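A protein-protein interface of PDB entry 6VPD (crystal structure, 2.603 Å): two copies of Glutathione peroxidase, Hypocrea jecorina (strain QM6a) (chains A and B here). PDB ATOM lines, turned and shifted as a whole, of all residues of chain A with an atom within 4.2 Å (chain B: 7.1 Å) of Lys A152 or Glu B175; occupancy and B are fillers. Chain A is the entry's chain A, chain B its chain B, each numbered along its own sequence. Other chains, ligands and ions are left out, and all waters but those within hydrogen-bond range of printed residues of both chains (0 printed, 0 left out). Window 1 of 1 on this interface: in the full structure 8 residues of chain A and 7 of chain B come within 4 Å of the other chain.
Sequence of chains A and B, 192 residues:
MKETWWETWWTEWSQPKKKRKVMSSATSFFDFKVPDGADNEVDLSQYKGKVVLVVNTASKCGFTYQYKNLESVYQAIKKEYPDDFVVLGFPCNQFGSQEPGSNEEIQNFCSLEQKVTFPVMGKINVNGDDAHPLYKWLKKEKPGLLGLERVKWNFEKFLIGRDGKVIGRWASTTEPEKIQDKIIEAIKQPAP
The backbone NH (N) of Lys A152 is in hydrogen-bond range of the side-chain carboxylate (OE1) of Glu A156. The side-chain hydroxyl (OH) of Tyr B65 sits at hydrogen-bond distance from the side-chain carboxylate (OE1) of Glu B175 (3.4 Å). The side-chain carboxylate (OE2) of Glu B175 sits at hydrogen-bond distance from the side-chain amide nitrogen (ND2) of Asn B69 (2.9 Å). The side-chain amide oxygen (OD1) of Asn B69 lies close to the side-chain carboxylate (OE2) of Glu B177 (2.7 Å). O of Glu B177 sits close to OE1 of Gln B180 (3.3 Å).
Among the printed residues, merely in contact across the chains: Leu A145 with Tyr B65, Lys A152 with Tyr B65, Lys A152 with Glu B175, Lys A152 with Glu B177, Trp A153 with Glu B177 and Trp A153 with Lys B178.
Of the printed residues of chain B, Leu A145 touches Tyr B65. Of chain B, only Tyr B65 (3.3 Å), Glu B175 (3.7 Å) and Glu B177 (3.8 Å) come within 4 Å of Lys A152. Ala A171 touches none of the printed residues of chain B. Gln B66 touches none of the printed residues of chain A. Printed residues of chain A within 4 Å of Glu B175: Lys A152 (3.7 Å). Printed residues of chain A within 4 Å of Glu B177: Lys A152 (3.8 Å) and Trp A153 (3.6 Å). The nearest residue of chain B that does not touch Lys A152 is Asn B69 (4.7 Å).
Of the 8 printed residues of chain A, 3 touch a printed residue of chain B. Hydrophobic or aromatic side chains of chain A that line the printed part of chain B: Leu A145 and Trp A153. Of the 17 printed residues of chain B, 4 touch a printed residue of chain A. Among the printed residues, no Asp or Glu carboxylate lies within 4 Å of a Lys or Arg side-chain nitrogen of the other chain.
Position printed for both chains: 171.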
ATOM      1  N   PHE A  95       5.610  -4.481  -1.838  1.00  0.00           N
ATOM      2  CA  PHE A  95       4.569  -3.646  -1.216  1.00  0.00           C
ATOM      3  C   PHE A  95       4.276  -4.145   0.207  1.00  0.00           C
ATOM      4  O   PHE A  95       3.169  -4.592   0.520  1.00  0.00           O
ATOM      5  CB  PHE A  95       3.290  -3.607  -2.081  1.00  0.00           C
ATOM      6  CG  PHE A  95       3.531  -3.135  -3.493  1.00  0.00           C
ATOM      7  CD1 PHE A  95       3.632  -1.782  -3.782  1.00  0.00           C
ATOM      8  CD2 PHE A  95       3.679  -4.054  -4.535  1.00  0.00           C
ATOM      9  CE1 PHE A  95       3.873  -1.355  -5.088  1.00  0.00           C
ATOM     10  CE2 PHE A  95       3.923  -3.636  -5.832  1.00  0.00           C
ATOM     11  CZ  PHE A  95       4.017  -2.291  -6.110  1.00  0.00           C
ATOM     12  N   LEU A 145      -2.547   6.700 -13.174  1.00  0.00           N
ATOM     13  CA  LEU A 145      -3.316   7.931 -13.081  1.00  0.00           C
ATOM     14  C   LEU A 145      -2.395   9.151 -13.070  1.00  0.00           C
ATOM     15  O   LEU A 145      -1.368   9.169 -12.375  1.00  0.00           O
ATOM     16  CB  LEU A 145      -4.188   7.876 -11.833  1.00  0.00           C
ATOM     17  CG  LEU A 145      -5.015   9.099 -11.476  1.00  0.00           C
ATOM     18  CD1 LEU A 145      -6.404   9.062 -12.146  1.00  0.00           C
ATOM     19  CD2 LEU A 145      -5.117   9.172  -9.964  1.00  0.00           C
ATOM     20  N   ARG A 150       4.716   4.188 -12.057  1.00  0.00           N
ATOM     21  CA  ARG A 150       4.851   3.175 -11.009  1.00  0.00           C
ATOM     22  C   ARG A 150       3.535   2.467 -10.694  1.00  0.00           C
ATOM     23  O   ARG A 150       2.458   3.077 -10.669  1.00  0.00           O
ATOM     24  CB  ARG A 150       5.395   3.802  -9.716  1.00  0.00           C
ATOM     25  CG  ARG A 150       6.873   4.253  -9.759  1.00  0.00           C
ATOM     26  CD  ARG A 150       7.788   3.031  -9.643  1.00  0.00           C
ATOM     27  NE  ARG A 150       9.156   3.218 -10.130  1.00  0.00           N
ATOM     28  CZ  ARG A 150       9.514   3.164 -11.408  1.00  0.00           C
ATOM     29  NH1 ARG A 150       8.585   2.919 -12.335  1.00  0.00           N
ATOM     30  NH2 ARG A 150      10.799   3.323 -11.726  1.00  0.00           N
ATOM     31  N   VAL A 151       3.645   1.160 -10.436  1.00  0.00           N
ATOM     32  CA  VAL A 151       2.579   0.422  -9.773  1.00  0.00           C
ATOM     33  C   VAL A 151       2.509   0.849  -8.316  1.00  0.00           C
ATOM     34  O   VAL A 151       3.513   0.832  -7.592  1.00  0.00           O
ATOM     35  CB  VAL A 151       2.816  -1.086  -9.903  1.00  0.00           C
ATOM     36  CG1 VAL A 151       1.717  -1.853  -9.198  1.00  0.00           C
ATOM     37  CG2 VAL A 151       2.889  -1.469 -11.379  1.00  0.00           C
ATOM     38  N   LYS A 152       1.318   1.234  -7.876  1.00  0.00           N
ATOM     39  CA  LYS A 152       1.162   1.806  -6.543  1.00  0.00           C
ATOM     40  C   LYS A 152       1.111   0.729  -5.468  1.00  0.00           C
ATOM     41  O   LYS A 152       1.713   0.892  -4.404  1.00  0.00           O
ATOM     42  CB  LYS A 152      -0.102   2.668  -6.490  1.00  0.00           C
ATOM     43  CG  LYS A 152      -0.183   3.693  -7.616  1.00  0.00           C
ATOM     44  CD  LYS A 152      -1.635   3.966  -8.053  1.00  0.00           C
ATOM     45  CE  LYS A 152      -1.729   4.217  -9.573  1.00  0.00           C
ATOM     46  NZ  LYS A 152      -3.139   4.369 -10.058  1.00  0.00           N
ATOM     47  N   TRP A 153       0.424  -0.381  -5.729  1.00  0.00           N
ATOM     48  CA  TRP A 153       0.145  -1.359  -4.689  1.00  0.00           C
ATOM     49  C   TRP A 153       0.051  -2.741  -5.329  1.00  0.00           C
ATOM     50  O   TRP A 153       0.169  -2.891  -6.553  1.00  0.00           O
ATOM     51  CB  TRP A 153      -1.130  -0.956  -3.946  1.00  0.00           C
ATOM     52  CG  TRP A 153      -1.386  -1.665  -2.649  1.00  0.00           C
ATOM     53  CD1 TRP A 153      -2.500  -2.398  -2.312  1.00  0.00           C
ATOM     54  CD2 TRP A 153      -0.521  -1.707  -1.506  1.00  0.00           C
ATOM     55  NE1 TRP A 153      -2.375  -2.889  -1.027  1.00  0.00           N
ATOM     56  CE2 TRP A 153      -1.168  -2.487  -0.515  1.00  0.00           C
ATOM     57  CE3 TRP A 153       0.745  -1.178  -1.229  1.00  0.00           C
ATOM     58  CZ2 TRP A 153      -0.589  -2.743   0.731  1.00  0.00           C
ATOM     59  CZ3 TRP A 153       1.326  -1.448   0.006  1.00  0.00           C
ATOM     60  CH2 TRP A 153       0.654  -2.211   0.974  1.00  0.00           C
ATOM     61  N   GLU A 156      -2.526  -4.249  -9.016  1.00  0.00           N
ATOM     62  CA  GLU A 156      -2.821  -3.516 -10.237  1.00  0.00           C
ATOM     63  C   GLU A 156      -2.951  -4.528 -11.375  1.00  0.00           C
ATOM     64  O   GLU A 156      -2.318  -5.591 -11.354  1.00  0.00           O
ATOM     65  CB  GLU A 156      -1.737  -2.463 -10.535  1.00  0.00           C
ATOM     66  CG  GLU A 156      -1.765  -1.221  -9.597  1.00  0.00           C
ATOM     67  CD  GLU A 156      -1.385   0.112 -10.282  1.00  0.00           C
ATOM     68  OE1 GLU A 156      -0.646   0.918  -9.672  1.00  0.00           O
ATOM     69  OE2 GLU A 156      -1.844   0.380 -11.417  1.00  0.00           O
ATOM     70  N   ALA A 171      -6.466   0.266 -11.064  1.00  0.00           N
ATOM     71  CA  ALA A 171      -5.790   0.313  -9.777  1.00  0.00           C
ATOM     72  C   ALA A 171      -6.201  -0.876  -8.915  1.00  0.00           C
ATOM     73  O   ALA A 171      -7.157  -1.599  -9.210  1.00  0.00           O
ATOM     74  CB  ALA A 171      -6.094   1.622  -9.065  1.00  0.00           C
ATOM     75  N   TYR B  65      -3.722  14.031  -7.597  1.00  0.00           N
ATOM     76  CA  TYR B  65      -3.330  12.640  -7.398  1.00  0.00           C
ATOM     77  C   TYR B  65      -3.793  12.142  -6.030  1.00  0.00           C
ATOM     78  O   TYR B  65      -4.291  11.015  -5.902  1.00  0.00           O
ATOM     79  CB  TYR B  65      -1.811  12.473  -7.556  1.00  0.00           C
ATOM     80  CG  TYR B  65      -1.410  11.019  -7.456  1.00  0.00           C
ATOM     81  CD1 TYR B  65      -1.543  10.161  -8.556  1.00  0.00           C
ATOM     82  CD2 TYR B  65      -0.970  10.479  -6.255  1.00  0.00           C
ATOM     83  CE1 TYR B  65      -1.218   8.808  -8.463  1.00  0.00           C
ATOM     84  CE2 TYR B  65      -0.643   9.134  -6.151  1.00  0.00           C
ATOM     85  CZ  TYR B  65      -0.771   8.302  -7.256  1.00  0.00           C
ATOM     86  OH  TYR B  65      -0.452   6.962  -7.154  1.00  0.00           O
ATOM     87  N   GLN B  66      -3.671  12.983  -5.007  1.00  0.00           N
ATOM     88  CA  GLN B  66      -3.999  12.571  -3.653  1.00  0.00           C
ATOM     89  C   GLN B  66      -5.517  12.472  -3.434  1.00  0.00           C
ATOM     90  O   GLN B  66      -5.975  11.570  -2.725  1.00  0.00           O
ATOM     91  CB  GLN B  66      -3.328  13.524  -2.655  1.00  0.00           C
ATOM     92  CG  GLN B  66      -1.768  13.655  -2.759  1.00  0.00           C
ATOM     93  CD  GLN B  66      -1.256  14.376  -4.035  1.00  0.00           C
ATOM     94  OE1 GLN B  66      -2.031  14.797  -4.897  1.00  0.00           O
ATOM     95  NE2 GLN B  66       0.057  14.522  -4.138  1.00  0.00           N
ATOM     96  N   ASN B  69      -6.775   9.268  -5.337  1.00  0.00           N
ATOM     97  CA  ASN B  69      -6.266   8.098  -4.635  1.00  0.00           C
ATOM     98  C   ASN B  69      -7.070   7.817  -3.369  1.00  0.00           C
ATOM     99  O   ASN B  69      -7.452   6.669  -3.105  1.00  0.00           O
ATOM    100  CB  ASN B  69      -4.791   8.325  -4.307  1.00  0.00           C
ATOM    101  CG  ASN B  69      -3.977   7.047  -4.350  1.00  0.00           C
ATOM    102  OD1 ASN B  69      -4.455   6.008  -4.823  1.00  0.00           O
ATOM    103  ND2 ASN B  69      -2.731   7.118  -3.863  1.00  0.00           N
ATOM    104  N   LEU B  70      -7.338   8.856  -2.579  1.00  0.00           N
ATOM    105  CA  LEU B  70      -8.131   8.690  -1.370  1.00  0.00           C
ATOM    106  C   LEU B  70      -9.552   8.284  -1.704  1.00  0.00           C
ATOM    107  O   LEU B  70     -10.074   7.318  -1.134  1.00  0.00           O
ATOM    108  CB  LEU B  70      -8.143   9.979  -0.540  1.00  0.00           C
ATOM    109  CG  LEU B  70      -7.083  10.024   0.558  1.00  0.00           C
ATOM    110  CD1 LEU B  70      -5.674  10.281  -0.028  1.00  0.00           C
ATOM    111  CD2 LEU B  70      -7.447  11.034   1.640  1.00  0.00           C
ATOM    112  N   VAL B  73      -9.707   4.640  -2.408  1.00  0.00           N
ATOM    113  CA  VAL B  73      -9.738   3.717  -1.278  1.00  0.00           C
ATOM    114  C   VAL B  73     -11.081   3.811  -0.551  1.00  0.00           C
ATOM    115  O   VAL B  73     -11.604   2.802  -0.062  1.00  0.00           O
ATOM    116  CB  VAL B  73      -8.538   3.983  -0.351  1.00  0.00           C
ATOM    117  CG1 VAL B  73      -8.549   3.031   0.841  1.00  0.00           C
ATOM    118  CG2 VAL B  73      -7.244   3.833  -1.137  1.00  0.00           C
ATOM    119  N   LYS B 157      -2.658  11.716   7.399  1.00  0.00           N
ATOM    120  CA  LYS B 157      -3.884  10.947   7.640  1.00  0.00           C
ATOM    121  C   LYS B 157      -3.949  10.431   9.078  1.00  0.00           C
ATOM    122  O   LYS B 157      -2.993   9.818   9.569  1.00  0.00           O
ATOM    123  CB  LYS B 157      -3.996   9.777   6.672  1.00  0.00           C
ATOM    124  CG  LYS B 157      -3.683  10.099   5.224  1.00  0.00           C
ATOM    125  CD  LYS B 157      -2.367   9.408   4.806  1.00  0.00           C
ATOM    126  CE  LYS B 157      -2.119   9.445   3.283  1.00  0.00           C
ATOM    127  NZ  LYS B 157      -1.869  10.784   2.676  1.00  0.00           N
ATOM    128  N   TRP B 170      -0.386   8.696   9.671  1.00  0.00           N
ATOM    129  CA  TRP B 170       0.555   8.504   8.574  1.00  0.00           C
ATOM    130  C   TRP B 170       0.809   9.845   7.915  1.00  0.00           C
ATOM    131  O   TRP B 170      -0.081  10.700   7.876  1.00  0.00           O
ATOM    132  CB  TRP B 170       0.032   7.510   7.514  1.00  0.00           C
ATOM    133  CG  TRP B 170      -0.212   6.143   8.054  1.00  0.00           C
ATOM    134  CD1 TRP B 170       0.623   5.074   7.969  1.00  0.00           C
ATOM    135  CD2 TRP B 170      -1.367   5.694   8.783  1.00  0.00           C
ATOM    136  NE1 TRP B 170       0.075   3.991   8.604  1.00  0.00           N
ATOM    137  CE2 TRP B 170      -1.147   4.344   9.117  1.00  0.00           C
ATOM    138  CE3 TRP B 170      -2.562   6.306   9.192  1.00  0.00           C
ATOM    139  CZ2 TRP B 170      -2.081   3.587   9.833  1.00  0.00           C
ATOM    140  CZ3 TRP B 170      -3.492   5.552   9.904  1.00  0.00           C
ATOM    141  CH2 TRP B 170      -3.248   4.209  10.212  1.00  0.00           C
ATOM    142  N   ALA B 171       2.020  10.018   7.384  1.00  0.00           N
ATOM    143  CA  ALA B 171       2.412  11.263   6.730  1.00  0.00           C
ATOM    144  C   ALA B 171       1.956  11.258   5.271  1.00  0.00           C
ATOM    145  O   ALA B 171       1.314  10.316   4.802  1.00  0.00           O
ATOM    146  CB  ALA B 171       3.921  11.474   6.849  1.00  0.00           C
ATOM    147  N   SER B 172       2.302  12.321   4.529  1.00  0.00           N
ATOM    148  CA  SER B 172       1.861  12.434   3.137  1.00  0.00           C
ATOM    149  C   SER B 172       2.501  11.395   2.223  1.00  0.00           C
ATOM    150  O   SER B 172       1.920  11.070   1.178  1.00  0.00           O
ATOM    151  CB  SER B 172       2.165  13.825   2.603  1.00  0.00           C
ATOM    152  OG  SER B 172       3.504  14.172   2.894  1.00  0.00           O
ATOM    153  N   THR B 173       3.669  10.856   2.604  1.00  0.00           N
ATOM    154  CA  THR B 173       4.411   9.874   1.810  1.00  0.00           C
ATOM    155  C   THR B 173       3.770   8.487   1.805  1.00  0.00           C
ATOM    156  O   THR B 173       4.139   7.654   0.968  1.00  0.00           O
ATOM    157  CB  THR B 173       5.862   9.751   2.321  1.00  0.00           C
ATOM    158  OG1 THR B 173       5.910   8.849   3.430  1.00  0.00           O
ATOM    159  CG2 THR B 173       6.425  11.105   2.772  1.00  0.00           C
ATOM    160  N   THR B 174       2.838   8.202   2.707  1.00  0.00           N
ATOM    161  CA  THR B 174       2.233   6.880   2.785  1.00  0.00           C
ATOM    162  C   THR B 174       0.999   6.813   1.895  1.00  0.00           C
ATOM    163  O   THR B 174       0.178   7.733   1.893  1.00  0.00           O
ATOM    164  CB  THR B 174       1.868   6.556   4.229  1.00  0.00           C
ATOM    165  OG1 THR B 174       3.069   6.323   4.963  1.00  0.00           O
ATOM    166  CG2 THR B 174       0.991   5.327   4.307  1.00  0.00           C
ATOM    167  N   GLU B 175       0.879   5.723   1.130  1.00  0.00           N
ATOM    168  CA  GLU B 175      -0.242   5.558   0.216  1.00  0.00           C
ATOM    169  C   GLU B 175      -1.492   5.125   0.979  1.00  0.00           C
ATOM    170  O   GLU B 175      -1.411   4.270   1.866  1.00  0.00           O
ATOM    171  CB  GLU B 175       0.085   4.524  -0.858  1.00  0.00           C
ATOM    172  CG  GLU B 175       0.947   5.061  -1.980  1.00  0.00           C
ATOM    173  CD  GLU B 175       0.172   5.961  -2.939  1.00  0.00           C
ATOM    174  OE1 GLU B 175      -0.097   5.532  -4.086  1.00  0.00           O
ATOM    175  OE2 GLU B 175      -0.173   7.096  -2.547  1.00  0.00           O
ATOM    176  N   PRO B 176      -2.652   5.690   0.645  1.00  0.00           N
ATOM    177  CA  PRO B 176      -3.909   5.206   1.236  1.00  0.00           C
ATOM    178  C   PRO B 176      -4.118   3.706   1.097  1.00  0.00           C
ATOM    179  O   PRO B 176      -4.728   3.095   1.984  1.00  0.00           O
ATOM    180  CB  PRO B 176      -4.989   5.981   0.461  1.00  0.00           C
ATOM    181  CG  PRO B 176      -4.298   7.093  -0.215  1.00  0.00           C
ATOM    182  CD  PRO B 176      -2.863   6.719  -0.386  1.00  0.00           C
ATOM    183  N   GLU B 177      -3.648   3.091   0.005  1.00  0.00           N
ATOM    184  CA  GLU B 177      -3.856   1.654  -0.185  1.00  0.00           C
ATOM    185  C   GLU B 177      -3.172   0.836   0.898  1.00  0.00           C
ATOM    186  O   GLU B 177      -3.585  -0.297   1.174  1.00  0.00           O
ATOM    187  CB  GLU B 177      -3.357   1.214  -1.561  1.00  0.00           C
ATOM    188  CG  GLU B 177      -4.077   1.891  -2.710  1.00  0.00           C
ATOM    189  CD  GLU B 177      -3.484   3.249  -3.039  1.00  0.00           C
ATOM    190  OE1 GLU B 177      -2.321   3.298  -3.505  1.00  0.00           O
ATOM    191  OE2 GLU B 177      -4.171   4.268  -2.812  1.00  0.00           O
ATOM    192  N   LYS B 178      -2.128   1.392   1.513  1.00  0.00           N
ATOM    193  CA  LYS B 178      -1.430   0.782   2.634  1.00  0.00           C
ATOM    194  C   LYS B 178      -2.203   0.866   3.944  1.00  0.00           C
ATOM    195  O   LYS B 178      -1.818   0.201   4.912  1.00  0.00           O
ATOM    196  CB  LYS B 178      -0.108   1.482   2.829  1.00  0.00           C
ATOM    197  CG  LYS B 178       0.799   1.372   1.668  1.00  0.00           C
ATOM    198  CD  LYS B 178       2.190   1.816   2.091  1.00  0.00           C
ATOM    199  CE  LYS B 178       2.468   1.551   3.585  1.00  0.00           C
ATOM    200  NZ  LYS B 178       3.885   1.833   3.857  1.00  0.00           N
ATOM    201  N   ILE B 179      -3.237   1.710   4.012  1.00  0.00           N
ATOM    202  CA  ILE B 179      -3.972   1.937   5.255  1.00  0.00           C
ATOM    203  C   ILE B 179      -5.172   1.005   5.362  1.00  0.00           C
ATOM    204  O   ILE B 179      -5.717   0.845   6.462  1.00  0.00           O
ATOM    205  CB  ILE B 179      -4.425   3.416   5.377  1.00  0.00           C
ATOM    206  CG1 ILE B 179      -3.248   4.380   5.253  1.00  0.00           C
ATOM    207  CG2 ILE B 179      -5.100   3.709   6.711  1.00  0.00           C
ATOM    208  CD1 ILE B 179      -3.614   5.819   5.590  1.00  0.00           C
ATOM    209  N   GLN B 180      -5.571   0.367   4.253  1.00  0.00           N
ATOM    210  CA  GLN B 180      -6.786  -0.441   4.219  1.00  0.00           C
ATOM    211  C   GLN B 180      -6.770  -1.547   5.260  1.00  0.00           C
ATOM    212  O   GLN B 180      -7.809  -1.850   5.855  1.00  0.00           O
ATOM    213  CB  GLN B 180      -6.976  -1.046   2.835  1.00  0.00           C
ATOM    214  CG  GLN B 180      -7.091  -0.007   1.752  1.00  0.00           C
ATOM    215  CD  GLN B 180      -7.345  -0.632   0.393  1.00  0.00           C
ATOM    216  OE1 GLN B 180      -6.400  -0.995  -0.318  1.00  0.00           O
ATOM    217  NE2 GLN B 180      -8.625  -0.760   0.020  1.00  0.00           N
